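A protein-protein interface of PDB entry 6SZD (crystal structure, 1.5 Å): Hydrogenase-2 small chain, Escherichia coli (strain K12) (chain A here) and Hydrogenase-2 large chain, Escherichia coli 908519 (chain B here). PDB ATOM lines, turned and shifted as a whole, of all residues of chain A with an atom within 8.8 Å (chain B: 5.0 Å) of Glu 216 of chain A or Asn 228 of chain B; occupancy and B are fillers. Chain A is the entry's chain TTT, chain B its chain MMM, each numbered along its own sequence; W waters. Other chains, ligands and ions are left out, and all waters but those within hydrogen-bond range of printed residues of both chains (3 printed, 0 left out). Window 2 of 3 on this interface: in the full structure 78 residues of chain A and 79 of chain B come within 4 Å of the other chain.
O of Ile 227 of chain B lies within hydrogen-bond range of NE of Arg 215 of chain A (2.7 Å).
The side-chain amide nitrogen of Asn 228 of chain B sits at hydrogen-bond distance from the backbone carbonyl oxygen of Arg 215 of chain A (3.1 Å).
OE2 of Glu 216 of chain A is in hydrogen-bond range of ND2 of Asn 228 of chain B, 3.3 Å away.
The backbone carbonyl oxygen of Gly 217 of chain A is in hydrogen-bond range of the guanidinium group of Arg 196 of chain A.
N of Gly 210 of chain A is in hydrogen-bond range of ND1 of His 214 of chain A (2.8 Å).
The side-chain carboxylate of Asp 211 of chain A lies within hydrogen-bond range of the backbone NH of His 214 of chain A.
The side-chain amide oxygen of Asn 228 of chain B lies close to the backbone NH of Asp 230 of chain B (3.1 Å).
The backbone NH (N) of Gly 231 of chain B sits at hydrogen-bond distance from the side-chain amide oxygen (OD1) of Asn 228 of chain B (3.4 Å).
The backbone NH of Asn 228 of chain B lies within hydrogen-bond range of the backbone carbonyl oxygen of Leu 235 of chain B (3.0 Å).
Among the printed residues, merely in contact across the chains: His 214 of chain A with Pro 226 of chain B, His 214 of chain A with Val 234 of chain B, Arg 215 of chain A with Pro 226 of chain B, Arg 215 of chain A with Val 234 of chain B, Glu 216 of chain A with Leu 232 of chain B and Gly 217 of chain A with Val 234 of chain B.
Printed residues of chain B within 4 Å of Arg 215 of chain A: Pro 226, Ile 227, Asn 228 and Val 234.
Glu 216 of chain A touches two residues of chain B.
Of the printed residues of chain B, Gly 217 of chain A touches Val 234.
Asn 228 of chain B touches just these residues of chain A: Arg 215 (3.1 Å) and Glu 216 (3.3 Å).
Printed residues of chain A within 4 Å of Leu 232 of chain B: Glu 216 (3.8 Å).
The nearest residue of chain B that does not touch Glu 216 of chain A is Val 234 of chain B (4.1 Å).
Of the 10 printed residues of chain B, 5 touch a printed residue of chain A.
Hydrophobic or aromatic side chains of chain B within 4 Å of the printed part of chain A: Pro 226 and Val 234.
Among the printed residues, no Asp or Glu carboxylate lies within 4 Å of a Lys or Arg side-chain nitrogen of the other chain.
Water W1 bridges OE2 of Glu 216 of chain A (2.5 Å) and ND2 of Asn 228 of chain B (3.0 Å).
Water W2 lies within hydrogen-bond range of OE1 of Glu 216 of chain A (2.7 Å) and O of Leu 232 of chain B (3.0 Å).
Water W3 bridges the side-chain carboxylate (OE1) of Glu 216 of chain A (2.8 Å) and the backbone carbonyl oxygen (O) of Asp 230 of chain B (3.2 Å).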
ATOM      1  N   ARG A 196       0.017  -2.283  20.985  1.00  0.00           N
ATOM      2  CA  ARG A 196       0.056  -3.763  20.951  1.00  0.00           C
ATOM      3  C   ARG A 196       1.226  -4.278  21.804  1.00  0.00           C
ATOM      4  O   ARG A 196       1.433  -5.505  21.856  1.00  0.00           O
ATOM      5  CB  ARG A 196       0.125  -4.281  19.512  1.00  0.00           C
ATOM      6  CG  ARG A 196      -1.061  -3.790  18.686  1.00  0.00           C
ATOM      7  CD  ARG A 196      -1.368  -4.613  17.495  1.00  0.00           C
ATOM      8  NE  ARG A 196      -2.600  -4.145  16.893  1.00  0.00           N
ATOM      9  CZ  ARG A 196      -3.258  -4.790  15.950  1.00  0.00           C
ATOM     10  NH1 ARG A 196      -2.827  -5.950  15.471  1.00  0.00           N
ATOM     11  NH2 ARG A 196      -4.402  -4.288  15.523  1.00  0.00           N
ATOM     12  N   HIS A 199       0.717  -7.288  24.018  1.00  0.00           N
ATOM     13  CA  HIS A 199       0.680  -8.596  23.309  1.00  0.00           C
ATOM     14  C   HIS A 199       2.117  -9.052  23.029  1.00  0.00           C
ATOM     15  O   HIS A 199       2.432 -10.224  23.294  1.00  0.00           O
ATOM     16  CB  HIS A 199      -0.126  -8.475  22.033  1.00  0.00           C
ATOM     17  CG  HIS A 199      -1.493  -7.975  22.304  1.00  0.00           C
ATOM     18  ND1 HIS A 199      -2.337  -8.603  23.206  1.00  0.00           N
ATOM     19  CD2 HIS A 199      -2.156  -6.914  21.800  1.00  0.00           C
ATOM     20  CE1 HIS A 199      -3.470  -7.925  23.237  1.00  0.00           C
ATOM     21  NE2 HIS A 199      -3.389  -6.884  22.385  1.00  0.00           N
ATOM     22  N   ARG A 204       1.909 -12.903  22.685  1.00  0.00           N
ATOM     23  CA  ARG A 204       0.689 -13.019  21.857  1.00  0.00           C
ATOM     24  C   ARG A 204       0.964 -12.406  20.472  1.00  0.00           C
ATOM     25  O   ARG A 204       0.890 -11.156  20.315  1.00  0.00           O
ATOM     26  CB  ARG A 204      -0.455 -12.317  22.577  1.00  0.00           C
ATOM     27  CG  ARG A 204      -0.947 -13.093  23.792  1.00  0.00           C
ATOM     28  CD  ARG A 204      -2.214 -12.524  24.360  1.00  0.00           C
ATOM     29  NE  ARG A 204      -2.104 -11.128  24.761  1.00  0.00           N
ATOM     30  CZ  ARG A 204      -2.016 -10.649  26.012  1.00  0.00           C
ATOM     31  NH1 ARG A 204      -1.968 -11.471  27.056  1.00  0.00           N
ATOM     32  NH2 ARG A 204      -1.997  -9.332  26.189  1.00  0.00           N
ATOM     33  N   PHE A 205       1.256 -13.252  19.501  1.00  0.00           N
ATOM     34  CA  PHE A 205       1.674 -12.839  18.133  1.00  0.00           C
ATOM     35  C   PHE A 205       0.741 -13.387  17.072  1.00  0.00           C
ATOM     36  O   PHE A 205       0.421 -14.585  17.079  1.00  0.00           O
ATOM     37  CB  PHE A 205       3.090 -13.347  17.870  1.00  0.00           C
ATOM     38  CG  PHE A 205       4.138 -12.793  18.781  1.00  0.00           C
ATOM     39  CD1 PHE A 205       4.503 -11.458  18.711  1.00  0.00           C
ATOM     40  CD2 PHE A 205       4.848 -13.619  19.654  1.00  0.00           C
ATOM     41  CE1 PHE A 205       5.467 -10.930  19.544  1.00  0.00           C
ATOM     42  CE2 PHE A 205       5.857 -13.099  20.446  1.00  0.00           C
ATOM     43  CZ  PHE A 205       6.175 -11.760  20.394  1.00  0.00           C
ATOM     44  N   ALA A 206       0.367 -12.547  16.107  1.00  0.00           N
ATOM     45  CA  ALA A 206      -0.198 -13.028  14.835  1.00  0.00           C
ATOM     46  C   ALA A 206       0.885 -13.814  14.109  1.00  0.00           C
ATOM     47  O   ALA A 206       2.047 -13.371  14.122  1.00  0.00           O
ATOM     48  CB  ALA A 206      -0.643 -11.868  13.992  1.00  0.00           C
ATOM     49  N   GLY A 210      -5.175 -13.170   9.071  1.00  0.00           N
ATOM     50  CA  GLY A 210      -6.427 -13.923   9.105  1.00  0.00           C
ATOM     51  C   GLY A 210      -6.438 -15.042  10.138  1.00  0.00           C
ATOM     52  O   GLY A 210      -7.519 -15.618  10.355  1.00  0.00           O
ATOM     53  N   ASP A 211      -5.328 -15.249  10.842  1.00  0.00           N
ATOM     54  CA  ASP A 211      -5.284 -16.308  11.887  1.00  0.00           C
ATOM     55  C   ASP A 211      -5.960 -15.772  13.148  1.00  0.00           C
ATOM     56  O   ASP A 211      -6.414 -14.592  13.199  1.00  0.00           O
ATOM     57  CB  ASP A 211      -3.870 -16.866  12.092  1.00  0.00           C
ATOM     58  CG  ASP A 211      -2.920 -16.080  12.983  1.00  0.00           C
ATOM     59  OD1 ASP A 211      -3.316 -14.997  13.535  1.00  0.00           O
ATOM     60  OD2 ASP A 211      -1.750 -16.525  13.094  1.00  0.00           O
ATOM     61  N   GLU A 212      -6.125 -16.655  14.140  1.00  0.00           N
ATOM     62  CA  GLU A 212      -6.963 -16.315  15.305  1.00  0.00           C
ATOM     63  C   GLU A 212      -6.342 -15.149  16.090  1.00  0.00           C
ATOM     64  O   GLU A 212      -7.101 -14.193  16.409  1.00  0.00           O
ATOM     65  CB  GLU A 212      -7.185 -17.605  16.095  1.00  0.00           C
ATOM     66  CG  GLU A 212      -8.084 -17.433  17.285  1.00  0.00           C
ATOM     67  CD  GLU A 212      -8.195 -18.759  18.040  1.00  0.00           C
ATOM     68  OE1 GLU A 212      -7.619 -18.858  19.153  1.00  0.00           O
ATOM     69  OE2 GLU A 212      -8.823 -19.687  17.487  1.00  0.00           O
ATOM     70  N   GLY A 213      -5.036 -15.126  16.304  1.00  0.00           N
ATOM     71  CA  GLY A 213      -4.338 -14.010  16.987  1.00  0.00           C
ATOM     72  C   GLY A 213      -4.480 -12.687  16.204  1.00  0.00           C
ATOM     73  O   GLY A 213      -4.747 -11.605  16.788  1.00  0.00           O
ATOM     74  N   HIS A 214      -4.289 -12.762  14.896  1.00  0.00           N
ATOM     75  CA  HIS A 214      -4.422 -11.565  14.018  1.00  0.00           C
ATOM     76  C   HIS A 214      -5.840 -10.995  14.176  1.00  0.00           C
ATOM     77  O   HIS A 214      -5.976  -9.737  14.288  1.00  0.00           O
ATOM     78  CB  HIS A 214      -4.137 -11.982  12.596  1.00  0.00           C
ATOM     79  CG  HIS A 214      -4.092 -10.831  11.644  1.00  0.00           C
ATOM     80  ND1 HIS A 214      -4.948 -10.766  10.570  1.00  0.00           N
ATOM     81  CD2 HIS A 214      -3.328  -9.716  11.620  1.00  0.00           C
ATOM     82  CE1 HIS A 214      -4.667  -9.666   9.885  1.00  0.00           C
ATOM     83  NE2 HIS A 214      -3.661  -9.025  10.499  1.00  0.00           N
ATOM     84  N   ARG A 215      -6.842 -11.865  14.240  1.00  0.00           N
ATOM     85  CA  ARG A 215      -8.266 -11.481  14.341  1.00  0.00           C
ATOM     86  C   ARG A 215      -8.609 -11.041  15.765  1.00  0.00           C
ATOM     87  O   ARG A 215      -9.756 -10.646  15.968  1.00  0.00           O
ATOM     88  CB  ARG A 215      -9.172 -12.570  13.765  1.00  0.00           C
ATOM     89  CG  ARG A 215      -9.042 -12.666  12.258  1.00  0.00           C
ATOM     90  CD  ARG A 215      -9.857 -13.807  11.665  1.00  0.00           C
ATOM     91  NE  ARG A 215     -11.245 -13.540  11.898  1.00  0.00           N
ATOM     92  CZ  ARG A 215     -12.065 -14.234  12.676  1.00  0.00           C
ATOM     93  NH1 ARG A 215     -11.635 -15.373  13.234  1.00  0.00           N
ATOM     94  NH2 ARG A 215     -13.318 -13.793  12.837  1.00  0.00           N
ATOM     95  N   GLU A 216      -7.657 -11.101  16.675  1.00  0.00           N
ATOM     96  CA  GLU A 216      -7.815 -10.542  18.041  1.00  0.00           C
ATOM     97  C   GLU A 216      -6.927  -9.320  18.252  1.00  0.00           C
ATOM     98  O   GLU A 216      -6.884  -8.805  19.360  1.00  0.00           O
ATOM     99  CB  GLU A 216      -7.564 -11.633  19.087  1.00  0.00           C
ATOM    100  CG  GLU A 216      -8.596 -12.765  19.066  1.00  0.00           C
ATOM    101  CD  GLU A 216     -10.081 -12.386  19.207  1.00  0.00           C
ATOM    102  OE1 GLU A 216     -10.440 -11.250  19.791  1.00  0.00           O
ATOM    103  OE2 GLU A 216     -10.919 -13.199  18.687  1.00  0.00           O
ATOM    104  N   GLY A 217      -6.289  -8.777  17.207  1.00  0.00           N
ATOM    105  CA  GLY A 217      -5.504  -7.537  17.341  1.00  0.00           C
ATOM    106  C   GLY A 217      -4.188  -7.740  18.062  1.00  0.00           C
ATOM    107  O   GLY A 217      -3.689  -6.834  18.690  1.00  0.00           O
ATOM    108  N   TRP A 218      -3.580  -8.929  17.954  1.00  0.00           N
ATOM    109  CA  TRP A 218      -2.301  -9.212  18.645  1.00  0.00           C
ATOM    110  C   TRP A 218      -1.128  -8.533  17.941  1.00  0.00           C
ATOM    111  O   TRP A 218      -1.260  -7.969  16.840  1.00  0.00           O
ATOM    112  CB  TRP A 218      -2.069 -10.723  18.754  1.00  0.00           C
ATOM    113  CG  TRP A 218      -2.970 -11.401  19.726  1.00  0.00           C
ATOM    114  CD1 TRP A 218      -3.913 -10.831  20.519  1.00  0.00           C
ATOM    115  CD2 TRP A 218      -2.957 -12.805  20.064  1.00  0.00           C
ATOM    116  NE1 TRP A 218      -4.509 -11.779  21.326  1.00  0.00           N
ATOM    117  CE2 TRP A 218      -3.938 -12.997  21.058  1.00  0.00           C
ATOM    118  CE3 TRP A 218      -2.181 -13.890  19.641  1.00  0.00           C
ATOM    119  CZ2 TRP A 218      -4.159 -14.244  21.639  1.00  0.00           C
ATOM    120  CZ3 TRP A 218      -2.418 -15.128  20.211  1.00  0.00           C
ATOM    121  CH2 TRP A 218      -3.388 -15.289  21.189  1.00  0.00           C
ATOM    122  N   CYS A 219       0.046  -8.627  18.527  1.00  0.00           N
ATOM    123  CA  CYS A 219       1.262  -7.958  18.037  1.00  0.00           C
ATOM    124  C   CYS A 219       1.679  -8.540  16.684  1.00  0.00           C
ATOM    125  O   CYS A 219       1.510  -9.780  16.488  1.00  0.00           O
ATOM    126  CB  CYS A 219       2.371  -8.054  19.086  1.00  0.00           C
ATOM    127  SG  CYS A 219       4.033  -7.629  18.523  1.00  0.00           S
ATOM    128  N   LEU A 220       2.236  -7.678  15.805  1.00  0.00           N
ATOM    129  CA  LEU A 220       2.611  -8.043  14.426  1.00  0.00           C
ATOM    130  C   LEU A 220       4.120  -8.254  14.278  1.00  0.00           C
ATOM    131  O   LEU A 220       4.586  -8.358  13.135  1.00  0.00           O
ATOM    132  CB  LEU A 220       2.071  -6.985  13.460  1.00  0.00           C
ATOM    133  CG  LEU A 220       0.569  -6.690  13.605  1.00  0.00           C
ATOM    134  CD1 LEU A 220       0.120  -5.712  12.516  1.00  0.00           C
ATOM    135  CD2 LEU A 220      -0.308  -7.940  13.601  1.00  0.00           C
ATOM    136  N   PRO B 226      -8.163  -7.838   9.472  1.00  0.00           N
ATOM    137  CA  PRO B 226      -8.707  -9.000  10.169  1.00  0.00           C
ATOM    138  C   PRO B 226     -10.216  -8.796  10.391  1.00  0.00           C
ATOM    139  O   PRO B 226     -10.605  -7.903  11.165  1.00  0.00           O
ATOM    140  CB  PRO B 226      -7.952  -8.982  11.512  1.00  0.00           C
ATOM    141  CG  PRO B 226      -7.141  -7.709  11.541  1.00  0.00           C
ATOM    142  CD  PRO B 226      -7.701  -6.837  10.438  1.00  0.00           C
ATOM    143  N   ILE B 227     -11.036  -9.580   9.713  1.00  0.00           N
ATOM    144  CA  ILE B 227     -12.508  -9.451   9.834  1.00  0.00           C
ATOM    145  C   ILE B 227     -12.947 -10.197  11.080  1.00  0.00           C
ATOM    146  O   ILE B 227     -12.778 -11.446  11.159  1.00  0.00           O
ATOM    147  CB  ILE B 227     -13.209  -9.960   8.595  1.00  0.00           C
ATOM    148  CG1 ILE B 227     -12.898  -9.053   7.399  1.00  0.00           C
ATOM    149  CG2 ILE B 227     -14.711 -10.105   8.879  1.00  0.00           C
ATOM    150  CD1 ILE B 227     -13.495  -9.515   6.107  1.00  0.00           C
ATOM    151  N   ASN B 228     -13.556  -9.483  12.024  1.00  0.00           N
ATOM    152  CA  ASN B 228     -14.123 -10.127  13.233  1.00  0.00           C
ATOM    153  C   ASN B 228     -15.132  -9.130  13.806  1.00  0.00           C
ATOM    154  O   ASN B 228     -14.710  -8.218  14.489  1.00  0.00           O
ATOM    155  CB  ASN B 228     -13.048 -10.493  14.241  1.00  0.00           C
ATOM    156  CG  ASN B 228     -13.565 -11.205  15.464  1.00  0.00           C
ATOM    157  OD1 ASN B 228     -14.772 -11.381  15.586  1.00  0.00           O
ATOM    158  ND2 ASN B 228     -12.654 -11.588  16.359  1.00  0.00           N
ATOM    159  N   LEU B 229     -16.406  -9.353  13.533  1.00  0.00           N
ATOM    160  CA  LEU B 229     -17.447  -8.411  14.028  1.00  0.00           C
ATOM    161  C   LEU B 229     -17.376  -8.273  15.529  1.00  0.00           C
ATOM    162  O   LEU B 229     -17.783  -7.201  16.019  1.00  0.00           O
ATOM    163  CB  LEU B 229     -18.832  -8.852  13.593  1.00  0.00           C
ATOM    164  CG  LEU B 229     -19.061  -8.841  12.091  1.00  0.00           C
ATOM    165  CD1 LEU B 229     -20.529  -8.989  11.809  1.00  0.00           C
ATOM    166  CD2 LEU B 229     -18.542  -7.585  11.419  1.00  0.00           C
ATOM    167  N   ASP B 230     -16.907  -9.303  16.242  1.00  0.00           N
ATOM    168  CA  ASP B 230     -16.889  -9.317  17.721  1.00  0.00           C
ATOM    169  C   ASP B 230     -15.519  -8.986  18.309  1.00  0.00           C
ATOM    170  O   ASP B 230     -15.375  -9.071  19.517  1.00  0.00           O
ATOM    171  CB  ASP B 230     -17.459 -10.649  18.197  1.00  0.00           C
ATOM    172  CG  ASP B 230     -18.904 -10.744  17.769  1.00  0.00           C
ATOM    173  OD1 ASP B 230     -19.702  -9.871  18.179  1.00  0.00           O
ATOM    174  OD2 ASP B 230     -19.194 -11.645  16.965  1.00  0.00           O
ATOM    175  N   GLY B 231     -14.562  -8.536  17.479  1.00  0.00           N
ATOM    176  CA  GLY B 231     -13.175  -8.347  17.865  1.00  0.00           C
ATOM    177  C   GLY B 231     -12.851  -6.911  18.231  1.00  0.00           C
ATOM    178  O   GLY B 231     -13.224  -6.003  17.496  1.00  0.00           O
ATOM    179  N   LEU B 232     -12.153  -6.713  19.334  1.00  0.00           N
ATOM    180  CA  LEU B 232     -11.598  -5.403  19.719  1.00  0.00           C
ATOM    181  C   LEU B 232     -10.347  -5.156  18.880  1.00  0.00           C
ATOM    182  O   LEU B 232      -9.520  -6.080  18.748  1.00  0.00           O
ATOM    183  CB  LEU B 232     -11.340  -5.448  21.222  1.00  0.00           C
ATOM    184  CG  LEU B 232     -10.903  -4.137  21.874  1.00  0.00           C
ATOM    185  CD1 LEU B 232     -11.415  -4.085  23.296  1.00  0.00           C
ATOM    186  CD2 LEU B 232      -9.395  -3.971  21.857  1.00  0.00           C
ATOM    187  N   VAL B 234      -9.860  -4.682  15.627  1.00  0.00           N
ATOM    188  CA  VAL B 234      -9.819  -5.249  14.254  1.00  0.00           C
ATOM    189  C   VAL B 234     -11.024  -4.731  13.463  1.00  0.00           C
ATOM    190  O   VAL B 234     -11.695  -3.762  13.932  1.00  0.00           O
ATOM    191  CB  VAL B 234      -9.767  -6.784  14.353  1.00  0.00           C
ATOM    192  CG1 VAL B 234      -8.537  -7.253  15.136  1.00  0.00           C
ATOM    193  CG2 VAL B 234     -11.022  -7.381  14.974  1.00  0.00           C
ATOM    194  N   LEU B 235     -11.263  -5.307  12.282  1.00  0.00           N
ATOM    195  CA  LEU B 235     -12.322  -4.804  11.369  1.00  0.00           C
ATOM    196  C   LEU B 235     -13.648  -5.402  11.848  1.00  0.00           C
ATOM    197  O   LEU B 235     -13.967  -6.542  11.496  1.00  0.00           O
ATOM    198  CB  LEU B 235     -12.014  -5.164   9.920  1.00  0.00           C
ATOM    199  CG  LEU B 235     -12.988  -4.614   8.887  1.00  0.00           C
ATOM    200  CD1 LEU B 235     -13.071  -3.108   8.984  1.00  0.00           C
ATOM    201  CD2 LEU B 235     -12.575  -4.991   7.497  1.00  0.00           C
ATOM    202  N   ASN B 236     -14.317  -4.647  12.706  1.00  0.00           N
ATOM    203  CA  ASN B 236     -15.549  -5.095  13.372  1.00  0.00           C
ATOM    204  C   ASN B 236     -16.737  -4.315  12.794  1.00  0.00           C
ATOM    205  O   ASN B 236     -16.596  -3.548  11.819  1.00  0.00           O
ATOM    206  CB  ASN B 236     -15.364  -5.046  14.875  1.00  0.00           C
ATOM    207  CG  ASN B 236     -15.117  -3.641  15.385  1.00  0.00           C
ATOM    208  OD1 ASN B 236     -15.532  -2.681  14.737  1.00  0.00           O
ATOM    209  ND2 ASN B 236     -14.438  -3.508  16.525  1.00  0.00           N
HETATM  210  O   HOH W   1     -13.420 -12.951  18.921  1.00  0.00           O
HETATM  211  O   HOH W   2     -10.025  -8.618  20.223  1.00  0.00           O
HETATM  212  O   HOH W   3     -13.176 -11.128  20.576  1.00  0.00           O
